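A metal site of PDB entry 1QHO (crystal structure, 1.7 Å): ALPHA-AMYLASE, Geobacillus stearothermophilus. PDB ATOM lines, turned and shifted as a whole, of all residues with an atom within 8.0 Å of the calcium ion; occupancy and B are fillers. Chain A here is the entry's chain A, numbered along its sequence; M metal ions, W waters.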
ATOM      1  N   PRO A 130       0.183  -1.355 -20.555  1.00  0.00           N
ATOM      2  CA  PRO A 130       0.658  -0.685 -21.751  1.00  0.00           C
ATOM      3  C   PRO A 130       2.029  -0.038 -21.701  1.00  0.00           C
ATOM      4  O   PRO A 130       2.515   0.458 -22.733  1.00  0.00           O
ATOM      5  CB  PRO A 130      -0.413   0.384 -22.097  1.00  0.00           C
ATOM      6  CG  PRO A 130      -0.924   0.709 -20.714  1.00  0.00           C
ATOM      7  CD  PRO A 130      -0.876  -0.584 -19.900  1.00  0.00           C
ATOM      8  N   ASN A 131       2.683  -0.010 -20.544  1.00  0.00           N
ATOM      9  CA  ASN A 131       3.972   0.676 -20.453  1.00  0.00           C
ATOM     10  C   ASN A 131       5.117  -0.061 -21.136  1.00  0.00           C
ATOM     11  O   ASN A 131       6.074   0.567 -21.587  1.00  0.00           O
ATOM     12  CB  ASN A 131       4.355   0.918 -18.987  1.00  0.00           C
ATOM     13  CG  ASN A 131       5.647   1.726 -18.911  1.00  0.00           C
ATOM     14  OD1 ASN A 131       5.585   2.864 -19.375  1.00  0.00           O
ATOM     15  ND2 ASN A 131       6.722   1.183 -18.370  1.00  0.00           N
ATOM     16  N   HIS A 132       5.061  -1.391 -21.165  1.00  0.00           N
ATOM     17  CA  HIS A 132       6.253  -2.112 -21.610  1.00  0.00           C
ATOM     18  C   HIS A 132       5.941  -3.515 -22.081  1.00  0.00           C
ATOM     19  O   HIS A 132       4.845  -4.013 -21.854  1.00  0.00           O
ATOM     20  CB  HIS A 132       7.242  -2.173 -20.428  1.00  0.00           C
ATOM     21  CG  HIS A 132       6.602  -2.624 -19.151  1.00  0.00           C
ATOM     22  ND1 HIS A 132       6.272  -1.720 -18.168  1.00  0.00           N
ATOM     23  CD2 HIS A 132       6.189  -3.843 -18.722  1.00  0.00           C
ATOM     24  CE1 HIS A 132       5.680  -2.352 -17.170  1.00  0.00           C
ATOM     25  NE2 HIS A 132       5.611  -3.627 -17.482  1.00  0.00           N
ATOM     26  N   HIS A 169      11.006   3.206 -26.757  1.00  0.00           N
ATOM     27  CA  HIS A 169      11.867   4.335 -26.410  1.00  0.00           C
ATOM     28  C   HIS A 169      13.277   3.780 -26.185  1.00  0.00           C
ATOM     29  O   HIS A 169      13.439   2.639 -25.785  1.00  0.00           O
ATOM     30  CB  HIS A 169      11.432   5.000 -25.092  1.00  0.00           C
ATOM     31  CG  HIS A 169      10.071   5.628 -25.165  1.00  0.00           C
ATOM     32  ND1 HIS A 169       9.170   5.498 -24.119  1.00  0.00           N
ATOM     33  CD2 HIS A 169       9.463   6.355 -26.139  1.00  0.00           C
ATOM     34  CE1 HIS A 169       8.057   6.147 -24.452  1.00  0.00           C
ATOM     35  NE2 HIS A 169       8.212   6.682 -25.666  1.00  0.00           N
ATOM     36  N   ILE A 174      15.432   4.397 -15.983  1.00  0.00           N
ATOM     37  CA  ILE A 174      15.051   5.392 -14.968  1.00  0.00           C
ATOM     38  C   ILE A 174      16.113   5.446 -13.870  1.00  0.00           C
ATOM     39  O   ILE A 174      16.522   4.386 -13.390  1.00  0.00           O
ATOM     40  CB  ILE A 174      13.696   5.030 -14.312  1.00  0.00           C
ATOM     41  CG1 ILE A 174      12.578   5.121 -15.372  1.00  0.00           C
ATOM     42  CG2 ILE A 174      13.394   5.938 -13.126  1.00  0.00           C
ATOM     43  CD1 ILE A 174      11.251   4.564 -14.879  1.00  0.00           C
ATOM     44  N   TYR A 181       9.970  13.323 -16.666  1.00  0.00           N
ATOM     45  CA  TYR A 181      10.466  12.888 -17.969  1.00  0.00           C
ATOM     46  C   TYR A 181      11.090  11.490 -17.857  1.00  0.00           C
ATOM     47  O   TYR A 181      10.767  10.616 -18.671  1.00  0.00           O
ATOM     48  CB  TYR A 181      11.472  13.897 -18.568  1.00  0.00           C
ATOM     49  CG  TYR A 181      12.070  13.336 -19.850  1.00  0.00           C
ATOM     50  CD1 TYR A 181      11.333  13.294 -21.014  1.00  0.00           C
ATOM     51  CD2 TYR A 181      13.336  12.764 -19.834  1.00  0.00           C
ATOM     52  CE1 TYR A 181      11.859  12.734 -22.170  1.00  0.00           C
ATOM     53  CE2 TYR A 181      13.874  12.207 -20.983  1.00  0.00           C
ATOM     54  CZ  TYR A 181      13.122  12.191 -22.132  1.00  0.00           C
ATOM     55  OH  TYR A 181      13.631  11.606 -23.272  1.00  0.00           O
ATOM     56  N   GLU A 182      11.948  11.253 -16.877  1.00  0.00           N
ATOM     57  CA  GLU A 182      12.547   9.925 -16.742  1.00  0.00           C
ATOM     58  C   GLU A 182      11.500   8.837 -16.501  1.00  0.00           C
ATOM     59  O   GLU A 182      11.520   7.789 -17.126  1.00  0.00           O
ATOM     60  CB  GLU A 182      13.555   9.823 -15.590  1.00  0.00           C
ATOM     61  CG  GLU A 182      14.784  10.713 -15.779  1.00  0.00           C
ATOM     62  CD  GLU A 182      15.851  10.382 -14.750  1.00  0.00           C
ATOM     63  OE1 GLU A 182      16.003   9.208 -14.391  1.00  0.00           O
ATOM     64  OE2 GLU A 182      16.528  11.319 -14.267  1.00  0.00           O
ATOM     65  N   ALA A 183      10.551   9.112 -15.603  1.00  0.00           N
ATOM     66  CA  ALA A 183       9.558   8.130 -15.225  1.00  0.00           C
ATOM     67  C   ALA A 183       8.734   7.650 -16.422  1.00  0.00           C
ATOM     68  O   ALA A 183       8.293   6.501 -16.417  1.00  0.00           O
ATOM     69  CB  ALA A 183       8.591   8.693 -14.171  1.00  0.00           C
ATOM     70  N   GLN A 184       8.548   8.521 -17.407  1.00  0.00           N
ATOM     71  CA  GLN A 184       7.748   8.175 -18.572  1.00  0.00           C
ATOM     72  C   GLN A 184       8.577   7.783 -19.780  1.00  0.00           C
ATOM     73  O   GLN A 184       8.101   6.938 -20.554  1.00  0.00           O
ATOM     74  CB  GLN A 184       6.834   9.364 -18.910  1.00  0.00           C
ATOM     75  CG  GLN A 184       5.788   9.649 -17.841  1.00  0.00           C
ATOM     76  CD  GLN A 184       5.101  10.986 -18.069  1.00  0.00           C
ATOM     77  OE1 GLN A 184       3.961  11.018 -18.544  1.00  0.00           O
ATOM     78  NE2 GLN A 184       5.790  12.080 -17.751  1.00  0.00           N
ATOM     79  N   TRP A 185       9.720   8.369 -20.053  1.00  0.00           N
ATOM     80  CA  TRP A 185      10.458   8.057 -21.275  1.00  0.00           C
ATOM     81  C   TRP A 185      11.640   7.135 -21.059  1.00  0.00           C
ATOM     82  O   TRP A 185      12.191   6.652 -22.068  1.00  0.00           O
ATOM     83  CB  TRP A 185      10.880   9.363 -22.003  1.00  0.00           C
ATOM     84  CG  TRP A 185       9.774   9.818 -22.931  1.00  0.00           C
ATOM     85  CD1 TRP A 185       9.642   9.508 -24.252  1.00  0.00           C
ATOM     86  CD2 TRP A 185       8.647  10.622 -22.584  1.00  0.00           C
ATOM     87  NE1 TRP A 185       8.483  10.055 -24.759  1.00  0.00           N
ATOM     88  CE2 TRP A 185       7.853  10.737 -23.745  1.00  0.00           C
ATOM     89  CE3 TRP A 185       8.217  11.248 -21.415  1.00  0.00           C
ATOM     90  CZ2 TRP A 185       6.655  11.470 -23.768  1.00  0.00           C
ATOM     91  CZ3 TRP A 185       7.025  11.965 -21.437  1.00  0.00           C
ATOM     92  CH2 TRP A 185       6.264  12.054 -22.601  1.00  0.00           C
ATOM     93  N   LYS A 186      12.023   6.859 -19.816  1.00  0.00           N
ATOM     94  CA  LYS A 186      13.127   5.936 -19.559  1.00  0.00           C
ATOM     95  C   LYS A 186      12.575   4.600 -19.076  1.00  0.00           C
ATOM     96  O   LYS A 186      11.375   4.473 -18.788  1.00  0.00           O
ATOM     97  CB  LYS A 186      14.163   6.529 -18.604  1.00  0.00           C
ATOM     98  CG  LYS A 186      14.878   7.731 -19.233  1.00  0.00           C
ATOM     99  CD  LYS A 186      16.022   8.214 -18.343  1.00  0.00           C
ATOM    100  CE  LYS A 186      16.659   9.435 -19.022  1.00  0.00           C
ATOM    101  NZ  LYS A 186      18.126   9.467 -18.777  1.00  0.00           N
ATOM    102  N   ASN A 187      13.432   3.573 -19.048  1.00  0.00           N
ATOM    103  CA  ASN A 187      12.976   2.227 -18.764  1.00  0.00           C
ATOM    104  C   ASN A 187      12.731   1.915 -17.297  1.00  0.00           C
ATOM    105  O   ASN A 187      13.536   2.164 -16.408  1.00  0.00           O
ATOM    106  CB  ASN A 187      13.989   1.185 -19.278  1.00  0.00           C
ATOM    107  CG  ASN A 187      14.524   1.509 -20.660  1.00  0.00           C
ATOM    108  OD1 ASN A 187      13.773   1.923 -21.536  1.00  0.00           O
ATOM    109  ND2 ASN A 187      15.829   1.321 -20.855  1.00  0.00           N
ATOM    110  N   PHE A 188      11.614   1.205 -17.096  1.00  0.00           N
ATOM    111  CA  PHE A 188      11.284   0.632 -15.791  1.00  0.00           C
ATOM    112  C   PHE A 188      12.370  -0.400 -15.482  1.00  0.00           C
ATOM    113  O   PHE A 188      12.740  -1.153 -16.376  1.00  0.00           O
ATOM    114  CB  PHE A 188       9.937  -0.089 -15.941  1.00  0.00           C
ATOM    115  CG  PHE A 188       9.207  -0.333 -14.659  1.00  0.00           C
ATOM    116  CD1 PHE A 188       9.610  -1.340 -13.796  1.00  0.00           C
ATOM    117  CD2 PHE A 188       8.100   0.440 -14.334  1.00  0.00           C
ATOM    118  CE1 PHE A 188       8.925  -1.562 -12.616  1.00  0.00           C
ATOM    119  CE2 PHE A 188       7.409   0.211 -13.153  1.00  0.00           C
ATOM    120  CZ  PHE A 188       7.825  -0.780 -12.291  1.00  0.00           C
ATOM    121  N   LEU A 196      12.730  -3.198 -18.403  1.00  0.00           N
ATOM    122  CA  LEU A 196      11.579  -3.606 -19.195  1.00  0.00           C
ATOM    123  C   LEU A 196      11.532  -2.717 -20.431  1.00  0.00           C
ATOM    124  O   LEU A 196      11.654  -1.495 -20.321  1.00  0.00           O
ATOM    125  CB  LEU A 196      10.283  -3.487 -18.376  1.00  0.00           C
ATOM    126  CG  LEU A 196      10.282  -4.193 -17.024  1.00  0.00           C
ATOM    127  CD1 LEU A 196       8.896  -4.105 -16.383  1.00  0.00           C
ATOM    128  CD2 LEU A 196      10.707  -5.655 -17.145  1.00  0.00           C
ATOM    129  N   ALA A 197      11.428  -3.317 -21.617  1.00  0.00           N
ATOM    130  CA  ALA A 197      11.440  -2.525 -22.865  1.00  0.00           C
ATOM    131  C   ALA A 197      10.254  -1.576 -22.911  1.00  0.00           C
ATOM    132  O   ALA A 197       9.109  -1.984 -22.851  1.00  0.00           O
ATOM    133  CB  ALA A 197      11.456  -3.468 -24.065  1.00  0.00           C
ATOM    134  N   ASP A 198      10.572  -0.284 -22.936  1.00  0.00           N
ATOM    135  CA  ASP A 198       9.540   0.746 -22.817  1.00  0.00           C
ATOM    136  C   ASP A 198       8.850   1.036 -24.143  1.00  0.00           C
ATOM    137  O   ASP A 198       9.489   1.523 -25.066  1.00  0.00           O
ATOM    138  CB  ASP A 198      10.279   1.991 -22.284  1.00  0.00           C
ATOM    139  CG  ASP A 198       9.318   2.895 -21.546  1.00  0.00           C
ATOM    140  OD1 ASP A 198       8.646   2.396 -20.599  1.00  0.00           O
ATOM    141  OD2 ASP A 198       9.196   4.096 -21.913  1.00  0.00           O
ATOM    142  N   LEU A 199       7.557   0.705 -24.229  1.00  0.00           N
ATOM    143  CA  LEU A 199       6.831   0.952 -25.475  1.00  0.00           C
ATOM    144  C   LEU A 199       6.676   2.438 -25.721  1.00  0.00           C
ATOM    145  O   LEU A 199       6.547   3.248 -24.803  1.00  0.00           O
ATOM    146  CB  LEU A 199       5.451   0.271 -25.389  1.00  0.00           C
ATOM    147  CG  LEU A 199       5.516  -1.264 -25.405  1.00  0.00           C
ATOM    148  CD1 LEU A 199       4.154  -1.812 -24.995  1.00  0.00           C
ATOM    149  CD2 LEU A 199       5.917  -1.769 -26.785  1.00  0.00           C
ATOM    150  N   SER A 200       6.668   2.790 -27.021  1.00  0.00           N
ATOM    151  CA  SER A 200       6.475   4.182 -27.413  1.00  0.00           C
ATOM    152  C   SER A 200       4.996   4.354 -27.758  1.00  0.00           C
ATOM    153  O   SER A 200       4.566   4.008 -28.859  1.00  0.00           O
ATOM    154  CB  SER A 200       7.331   4.549 -28.628  1.00  0.00           C
ATOM    155  OG  SER A 200       7.127   5.930 -28.927  1.00  0.00           O
ATOM    156  N   GLN A 201       4.216   4.893 -26.818  1.00  0.00           N
ATOM    157  CA  GLN A 201       2.805   5.182 -27.077  1.00  0.00           C
ATOM    158  C   GLN A 201       2.662   6.375 -28.031  1.00  0.00           C
ATOM    159  O   GLN A 201       1.542   6.631 -28.489  1.00  0.00           O
ATOM    160  CB  GLN A 201       2.005   5.443 -25.800  1.00  0.00           C
ATOM    161  CG  GLN A 201       2.017   4.251 -24.828  1.00  0.00           C
ATOM    162  CD  GLN A 201       3.266   4.210 -23.977  1.00  0.00           C
ATOM    163  OE1 GLN A 201       4.041   5.172 -23.914  1.00  0.00           O
ATOM    164  NE2 GLN A 201       3.463   3.086 -23.268  1.00  0.00           N
ATOM    165  N   GLU A 202       3.741   7.069 -28.343  1.00  0.00           N
ATOM    166  CA  GLU A 202       3.735   8.184 -29.293  1.00  0.00           C
ATOM    167  C   GLU A 202       3.935   7.652 -30.716  1.00  0.00           C
ATOM    168  O   GLU A 202       3.861   8.402 -31.687  1.00  0.00           O
ATOM    169  CB  GLU A 202       4.791   9.228 -28.925  1.00  0.00           C
ATOM    170  CG  GLU A 202       4.637   9.762 -27.499  1.00  0.00           C
ATOM    171  CD  GLU A 202       5.245   8.864 -26.439  1.00  0.00           C
ATOM    172  OE1 GLU A 202       6.168   8.093 -26.743  1.00  0.00           O
ATOM    173  OE2 GLU A 202       4.788   8.919 -25.278  1.00  0.00           O
ATOM    174  N   ALA A 229       0.669   1.246 -14.157  1.00  0.00           N
ATOM    175  CA  ALA A 229       1.726   2.232 -14.291  1.00  0.00           C
ATOM    176  C   ALA A 229       1.371   3.442 -15.145  1.00  0.00           C
ATOM    177  O   ALA A 229       2.113   3.840 -16.040  1.00  0.00           O
ATOM    178  CB  ALA A 229       2.909   1.481 -14.927  1.00  0.00           C
ATOM    179  N   LYS A 231       1.544   6.503 -14.378  1.00  0.00           N
ATOM    180  CA  LYS A 231       2.495   7.602 -14.208  1.00  0.00           C
ATOM    181  C   LYS A 231       3.732   7.374 -15.071  1.00  0.00           C
ATOM    182  O   LYS A 231       4.600   8.234 -15.113  1.00  0.00           O
ATOM    183  CB  LYS A 231       2.880   7.717 -12.734  1.00  0.00           C
ATOM    184  CG  LYS A 231       3.855   6.682 -12.204  1.00  0.00           C
ATOM    185  CD  LYS A 231       3.963   6.709 -10.680  1.00  0.00           C
ATOM    186  CE  LYS A 231       4.768   7.878 -10.166  1.00  0.00           C
ATOM    187  NZ  LYS A 231       5.084   7.705  -8.707  1.00  0.00           N
ATOM    188  N   HIS A 232       3.845   6.216 -15.717  1.00  0.00           N
ATOM    189  CA  HIS A 232       5.001   5.853 -16.516  1.00  0.00           C
ATOM    190  C   HIS A 232       4.762   5.978 -18.002  1.00  0.00           C
ATOM    191  O   HIS A 232       5.720   5.770 -18.731  1.00  0.00           O
ATOM    192  CB  HIS A 232       5.456   4.410 -16.157  1.00  0.00           C
ATOM    193  CG  HIS A 232       5.971   4.385 -14.742  1.00  0.00           C
ATOM    194  ND1 HIS A 232       7.128   5.062 -14.385  1.00  0.00           N
ATOM    195  CD2 HIS A 232       5.483   3.821 -13.617  1.00  0.00           C
ATOM    196  CE1 HIS A 232       7.307   4.909 -13.072  1.00  0.00           C
ATOM    197  NE2 HIS A 232       6.331   4.148 -12.583  1.00  0.00           N
ATOM    198  N   PHE A 233       3.616   6.402 -18.509  1.00  0.00           N
ATOM    199  CA  PHE A 233       3.471   6.647 -19.960  1.00  0.00           C
ATOM    200  C   PHE A 233       2.671   7.953 -20.059  1.00  0.00           C
ATOM    201  O   PHE A 233       1.943   8.290 -19.114  1.00  0.00           O
ATOM    202  CB  PHE A 233       2.898   5.488 -20.725  1.00  0.00           C
ATOM    203  CG  PHE A 233       1.517   5.079 -20.315  1.00  0.00           C
ATOM    204  CD1 PHE A 233       1.325   4.131 -19.316  1.00  0.00           C
ATOM    205  CD2 PHE A 233       0.402   5.636 -20.945  1.00  0.00           C
ATOM    206  CE1 PHE A 233       0.049   3.768 -18.928  1.00  0.00           C
ATOM    207  CE2 PHE A 233      -0.876   5.260 -20.564  1.00  0.00           C
ATOM    208  CZ  PHE A 233      -1.044   4.332 -19.560  1.00  0.00           C
ATOM    209  N   ASN A 234       2.830   8.681 -21.167  1.00  0.00           N
ATOM    210  CA  ASN A 234       2.158   9.978 -21.254  1.00  0.00           C
ATOM    211  C   ASN A 234       0.666   9.924 -20.966  1.00  0.00           C
ATOM    212  O   ASN A 234      -0.021   8.977 -21.327  1.00  0.00           O
ATOM    213  CB  ASN A 234       2.508  10.660 -22.582  1.00  0.00           C
ATOM    214  CG  ASN A 234       1.619  10.256 -23.747  1.00  0.00           C
ATOM    215  OD1 ASN A 234       0.463  10.681 -23.764  1.00  0.00           O
ATOM    216  ND2 ASN A 234       2.129   9.481 -24.695  1.00  0.00           N
HETATM  217 CA    CA M   1       7.128   4.580 -20.423  1.00  0.00          CA
HETATM  218  O   HOH W   1       5.871   5.928 -22.176  1.00  0.00           O
HETATM  219  O   HOH W   2       6.135   3.059 -22.218  1.00  0.00           O
HETATM  220  O   HOH W   3       8.662   4.537 -18.381  1.00  0.00           O
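O of Ala 183 is in hydrogen-bond range of ND1 of His 232 (2.7 Å). The backbone carbonyl oxygen of Asn 131 sits at hydrogen-bond distance from the backbone NH of Leu 199, 3.0 Å away. A ring nitrogen (ND1) of His 132 sits at hydrogen-bond distance from the side-chain amide nitrogen of Asn 131, 2.9 Å away. The backbone carbonyl oxygen of Phe 233 lies close to the side-chain amide oxygen of Gln 184, at 3.4 Å. The backbone carbonyl oxygen (O) of Asp 198 is in hydrogen-bond range of the backbone NH (N) of His 169 (2.8 Å).
The backbone carbonyl oxygen (O) of His 232 binds the calcium ion (2.5 Å). The calcium ion is bound by the side-chain amide oxygen (OD1) of Asn 131 (2.5 Å). Water W1 binds the calcium ion, 2.5 Å away. The calcium ion is bound by water W2, 2.6 Å away. Water W3 is bound to the calcium ion (2.6 Å). O of Gln 184 binds the calcium ion, 2.6 Å away. OD2 of Asp 198 is bound to the calcium ion (2.6 Å). The calcium ion is bound by OD1 of Asp 198.
Within 4 Å of the calcium ion: Asn 131, Gln 184, Asp 198 and His 232. The nearest printed residue that does not touch the calcium ion is Phe 233 (4.2 Å).
Water W2 lies within hydrogen-bond range of O of Asn 131 (2.6 Å), O of Leu 199 (2.6 Å) and NE2 of Gln 201 (2.9 Å).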
